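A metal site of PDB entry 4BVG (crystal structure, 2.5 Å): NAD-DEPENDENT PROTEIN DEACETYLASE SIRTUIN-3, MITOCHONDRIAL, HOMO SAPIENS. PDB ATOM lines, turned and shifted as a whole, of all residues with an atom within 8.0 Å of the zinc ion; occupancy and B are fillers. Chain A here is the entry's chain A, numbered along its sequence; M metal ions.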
ATOM      1  N   THR A 140      -4.192 -29.822  31.863  1.00  0.00           N
ATOM      2  CA  THR A 140      -3.053 -29.672  30.943  1.00  0.00           C
ATOM      3  C   THR A 140      -3.547 -29.381  29.554  1.00  0.00           C
ATOM      4  O   THR A 140      -4.503 -30.004  29.065  1.00  0.00           O
ATOM      5  CB  THR A 140      -2.201 -30.977  30.901  1.00  0.00           C
ATOM      6  OG1 THR A 140      -1.893 -31.343  32.248  1.00  0.00           O
ATOM      7  CG2 THR A 140      -0.852 -30.800  30.061  1.00  0.00           C
ATOM      8  N   CYS A 141      -2.914 -28.411  28.902  1.00  0.00           N
ATOM      9  CA  CYS A 141      -3.229 -28.135  27.516  1.00  0.00           C
ATOM     10  C   CYS A 141      -2.787 -29.332  26.703  1.00  0.00           C
ATOM     11  O   CYS A 141      -1.626 -29.820  26.838  1.00  0.00           O
ATOM     12  CB  CYS A 141      -2.506 -26.900  27.020  1.00  0.00           C
ATOM     13  SG  CYS A 141      -2.627 -26.727  25.229  1.00  0.00           S
ATOM     14  N   THR A 142      -3.680 -29.798  25.835  1.00  0.00           N
ATOM     15  CA  THR A 142      -3.369 -30.985  25.034  1.00  0.00           C
ATOM     16  C   THR A 142      -2.369 -30.738  23.889  1.00  0.00           C
ATOM     17  O   THR A 142      -1.882 -31.676  23.238  1.00  0.00           O
ATOM     18  CB  THR A 142      -4.632 -31.522  24.392  1.00  0.00           C
ATOM     19  OG1 THR A 142      -5.201 -30.457  23.566  1.00  0.00           O
ATOM     20  CG2 THR A 142      -5.565 -32.046  25.484  1.00  0.00           C
ATOM     21  N   VAL A 143      -2.079 -29.471  23.610  1.00  0.00           N
ATOM     22  CA  VAL A 143      -1.144 -29.149  22.526  1.00  0.00           C
ATOM     23  C   VAL A 143       0.268 -28.787  23.021  1.00  0.00           C
ATOM     24  O   VAL A 143       1.251 -29.352  22.562  1.00  0.00           O
ATOM     25  CB  VAL A 143      -1.755 -28.090  21.621  1.00  0.00           C
ATOM     26  CG1 VAL A 143      -0.695 -27.573  20.631  1.00  0.00           C
ATOM     27  CG2 VAL A 143      -2.969 -28.682  20.885  1.00  0.00           C
ATOM     28  N   CYS A 144       0.343 -27.877  23.970  1.00  0.00           N
ATOM     29  CA  CYS A 144       1.619 -27.285  24.343  1.00  0.00           C
ATOM     30  C   CYS A 144       2.019 -27.784  25.717  1.00  0.00           C
ATOM     31  O   CYS A 144       3.055 -27.401  26.215  1.00  0.00           O
ATOM     32  CB  CYS A 144       1.520 -25.745  24.379  1.00  0.00           C
ATOM     33  SG  CYS A 144       0.461 -25.062  25.689  1.00  0.00           S
ATOM     34  N   GLN A 145       1.160 -28.610  26.317  1.00  0.00           N
ATOM     35  CA  GLN A 145       1.350 -29.171  27.673  1.00  0.00           C
ATOM     36  C   GLN A 145       1.526 -28.162  28.864  1.00  0.00           C
ATOM     37  O   GLN A 145       1.929 -28.561  29.958  1.00  0.00           O
ATOM     38  CB  GLN A 145       2.422 -30.310  27.691  1.00  0.00           C
ATOM     39  CG  GLN A 145       2.565 -31.137  26.396  1.00  0.00           C
ATOM     40  CD  GLN A 145       1.269 -31.801  25.920  1.00  0.00           C
ATOM     41  OE1 GLN A 145       0.522 -32.401  26.722  1.00  0.00           O
ATOM     42  NE2 GLN A 145       0.987 -31.713  24.606  1.00  0.00           N
ATOM     43  N   ARG A 146       1.187 -26.885  28.670  1.00  0.00           N
ATOM     44  CA  ARG A 146       1.200 -25.951  29.814  1.00  0.00           C
ATOM     45  C   ARG A 146       0.169 -26.446  30.874  1.00  0.00           C
ATOM     46  O   ARG A 146      -0.939 -26.823  30.489  1.00  0.00           O
ATOM     47  CB  ARG A 146       0.917 -24.506  29.362  1.00  0.00           C
ATOM     48  CG  ARG A 146       0.971 -23.465  30.472  1.00  0.00           C
ATOM     49  CD  ARG A 146       0.961 -22.028  29.952  1.00  0.00           C
ATOM     50  NE  ARG A 146       1.412 -21.075  30.970  1.00  0.00           N
ATOM     51  CZ  ARG A 146       0.712 -20.017  31.384  1.00  0.00           C
ATOM     52  NH1 ARG A 146      -0.481 -19.736  30.873  1.00  0.00           N
ATOM     53  NH2 ARG A 146       1.206 -19.240  32.308  1.00  0.00           N
ATOM     54  N   PRO A 147       0.554 -26.502  32.179  1.00  0.00           N
ATOM     55  CA  PRO A 147      -0.362 -26.953  33.252  1.00  0.00           C
ATOM     56  C   PRO A 147      -1.181 -25.790  33.798  1.00  0.00           C
ATOM     57  O   PRO A 147      -0.691 -24.668  33.834  1.00  0.00           O
ATOM     58  CB  PRO A 147       0.600 -27.440  34.330  1.00  0.00           C
ATOM     59  CG  PRO A 147       1.698 -26.418  34.268  1.00  0.00           C
ATOM     60  CD  PRO A 147       1.890 -26.221  32.761  1.00  0.00           C
ATOM     61  N   PHE A 148      -2.397 -26.056  34.204  1.00  0.00           N
ATOM     62  CA  PHE A 148      -3.284 -25.026  34.736  1.00  0.00           C
ATOM     63  C   PHE A 148      -3.937 -25.612  35.987  1.00  0.00           C
ATOM     64  O   PHE A 148      -4.210 -26.837  36.016  1.00  0.00           O
ATOM     65  CB  PHE A 148      -4.386 -24.689  33.720  1.00  0.00           C
ATOM     66  CG  PHE A 148      -3.894 -24.042  32.433  1.00  0.00           C
ATOM     67  CD1 PHE A 148      -3.526 -24.825  31.339  1.00  0.00           C
ATOM     68  CD2 PHE A 148      -3.833 -22.669  32.302  1.00  0.00           C
ATOM     69  CE1 PHE A 148      -3.090 -24.243  30.146  1.00  0.00           C
ATOM     70  CE2 PHE A 148      -3.379 -22.073  31.115  1.00  0.00           C
ATOM     71  CZ  PHE A 148      -3.021 -22.870  30.035  1.00  0.00           C
ATOM     72  N   ARG A 164     -10.001 -23.597  26.551  1.00  0.00           N
ATOM     73  CA  ARG A 164      -8.806 -23.532  25.682  1.00  0.00           C
ATOM     74  C   ARG A 164      -7.585 -22.810  26.286  1.00  0.00           C
ATOM     75  O   ARG A 164      -7.696 -22.064  27.258  1.00  0.00           O
ATOM     76  CB  ARG A 164      -9.177 -23.005  24.301  1.00  0.00           C
ATOM     77  CG  ARG A 164     -10.077 -24.009  23.566  1.00  0.00           C
ATOM     78  CD  ARG A 164     -10.670 -23.436  22.312  1.00  0.00           C
ATOM     79  NE  ARG A 164     -11.405 -24.453  21.551  1.00  0.00           N
ATOM     80  CZ  ARG A 164     -10.861 -25.335  20.734  1.00  0.00           C
ATOM     81  NH1 ARG A 164      -9.557 -25.403  20.529  1.00  0.00           N
ATOM     82  NH2 ARG A 164     -11.628 -26.181  20.111  1.00  0.00           N
ATOM     83  N   CYS A 165      -6.414 -23.144  25.768  1.00  0.00           N
ATOM     84  CA  CYS A 165      -5.156 -22.586  26.194  1.00  0.00           C
ATOM     85  C   CYS A 165      -5.082 -21.111  25.750  1.00  0.00           C
ATOM     86  O   CYS A 165      -5.176 -20.838  24.571  1.00  0.00           O
ATOM     87  CB  CYS A 165      -4.049 -23.372  25.516  1.00  0.00           C
ATOM     88  SG  CYS A 165      -2.406 -23.125  26.183  1.00  0.00           S
ATOM     89  N   PRO A 166      -4.923 -20.156  26.696  1.00  0.00           N
ATOM     90  CA  PRO A 166      -4.583 -18.763  26.345  1.00  0.00           C
ATOM     91  C   PRO A 166      -3.324 -18.580  25.456  1.00  0.00           C
ATOM     92  O   PRO A 166      -3.210 -17.552  24.775  1.00  0.00           O
ATOM     93  CB  PRO A 166      -4.366 -18.090  27.718  1.00  0.00           C
ATOM     94  CG  PRO A 166      -4.094 -19.237  28.681  1.00  0.00           C
ATOM     95  CD  PRO A 166      -4.920 -20.381  28.160  1.00  0.00           C
ATOM     96  N   VAL A 167      -2.412 -19.558  25.393  1.00  0.00           N
ATOM     97  CA  VAL A 167      -1.180 -19.366  24.666  1.00  0.00           C
ATOM     98  C   VAL A 167      -1.291 -19.972  23.257  1.00  0.00           C
ATOM     99  O   VAL A 167      -0.923 -19.307  22.280  1.00  0.00           O
ATOM    100  CB  VAL A 167       0.071 -19.926  25.429  1.00  0.00           C
ATOM    101  CG1 VAL A 167       1.330 -19.758  24.574  1.00  0.00           C
ATOM    102  CG2 VAL A 167       0.269 -19.246  26.766  1.00  0.00           C
ATOM    103  N   CYS A 168      -1.756 -21.218  23.138  1.00  0.00           N
ATOM    104  CA  CYS A 168      -1.763 -21.876  21.827  1.00  0.00           C
ATOM    105  C   CYS A 168      -3.158 -22.177  21.227  1.00  0.00           C
ATOM    106  O   CYS A 168      -3.249 -22.601  20.068  1.00  0.00           O
ATOM    107  CB  CYS A 168      -0.932 -23.152  21.842  1.00  0.00           C
ATOM    108  SG  CYS A 168      -1.788 -24.551  22.605  1.00  0.00           S
ATOM    109  N   THR A 169      -4.217 -21.909  22.019  1.00  0.00           N
ATOM    110  CA  THR A 169      -5.633 -22.119  21.698  1.00  0.00           C
ATOM    111  C   THR A 169      -6.080 -23.583  21.716  1.00  0.00           C
ATOM    112  O   THR A 169      -7.246 -23.854  21.456  1.00  0.00           O
ATOM    113  CB  THR A 169      -6.101 -21.490  20.346  1.00  0.00           C
ATOM    114  OG1 THR A 169      -5.560 -22.209  19.216  1.00  0.00           O
ATOM    115  CG2 THR A 169      -5.815 -19.988  20.254  1.00  0.00           C
ATOM    116  N   GLY A 170      -5.156 -24.513  21.939  1.00  0.00           N
ATOM    117  CA  GLY A 170      -5.481 -25.934  22.128  1.00  0.00           C
ATOM    118  C   GLY A 170      -6.455 -26.226  23.258  1.00  0.00           C
ATOM    119  O   GLY A 170      -6.649 -25.398  24.171  1.00  0.00           O
ATOM    120  N   VAL A 171      -7.106 -27.385  23.178  1.00  0.00           N
ATOM    121  CA  VAL A 171      -8.091 -27.806  24.198  1.00  0.00           C
ATOM    122  C   VAL A 171      -7.283 -28.146  25.455  1.00  0.00           C
ATOM    123  O   VAL A 171      -6.245 -28.853  25.373  1.00  0.00           O
ATOM    124  CB  VAL A 171      -8.979 -29.041  23.748  1.00  0.00           C
ATOM    125  CG1 VAL A 171      -9.831 -29.573  24.923  1.00  0.00           C
ATOM    126  CG2 VAL A 171      -9.884 -28.708  22.523  1.00  0.00           C
ATOM    127  N   VAL A 172      -7.781 -27.681  26.575  1.00  0.00           N
ATOM    128  CA  VAL A 172      -7.247 -27.943  27.893  1.00  0.00           C
ATOM    129  C   VAL A 172      -8.059 -29.001  28.559  1.00  0.00           C
ATOM    130  O   VAL A 172      -9.220 -28.882  28.664  1.00  0.00           O
ATOM    131  CB  VAL A 172      -7.288 -26.695  28.759  1.00  0.00           C
ATOM    132  CG1 VAL A 172      -6.712 -26.973  30.117  1.00  0.00           C
ATOM    133  CG2 VAL A 172      -6.523 -25.599  28.107  1.00  0.00           C
HETATM  134 ZN    ZN M   1      -1.460 -24.635  24.837  1.00  0.00          ZN
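The backbone NH (N) of Arg 146 sits close to the side-chain sulfur (SG) of Cys 144, 3.6 Å away. The backbone NH of Cys 165 lies within hydrogen-bond range of the backbone carbonyl oxygen of Gly 170, at 2.8 Å. The backbone NH (N) of Val 167 sits close to the side-chain sulfur (SG) of Cys 165, 3.7 Å away. The side-chain sulfur (SG) of Cys 168 lies close to the backbone NH (N) of Gly 170 (3.4 Å). SG of Cys 141 sits close to N of Val 143, at 3.2 Å. The side-chain amide oxygen (OE1) of Gln 145 sits close to the backbone carbonyl oxygen (O) of Cys 141 (3.4 Å). The backbone carbonyl oxygen (O) of Arg 146 sits at hydrogen-bond distance from the backbone NH (N) of Cys 141, at 3.0 Å.
The zinc ion is bound by the side-chain sulfur (SG) of Cys 144, at 2.1 Å. The side-chain sulfur (SG) of Cys 165 binds the zinc ion, at 2.2 Å. The side-chain sulfur (SG) of Cys 168 binds the zinc ion (2.3 Å). The zinc ion is bound by the side-chain sulfur (SG) of Cys 141 (2.4 Å).
Of the 18 residues printed, 4 come within 4 Å of the zinc ion. Along chain A the residues within 4 Å of the zinc ion span positions 141 to 168.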
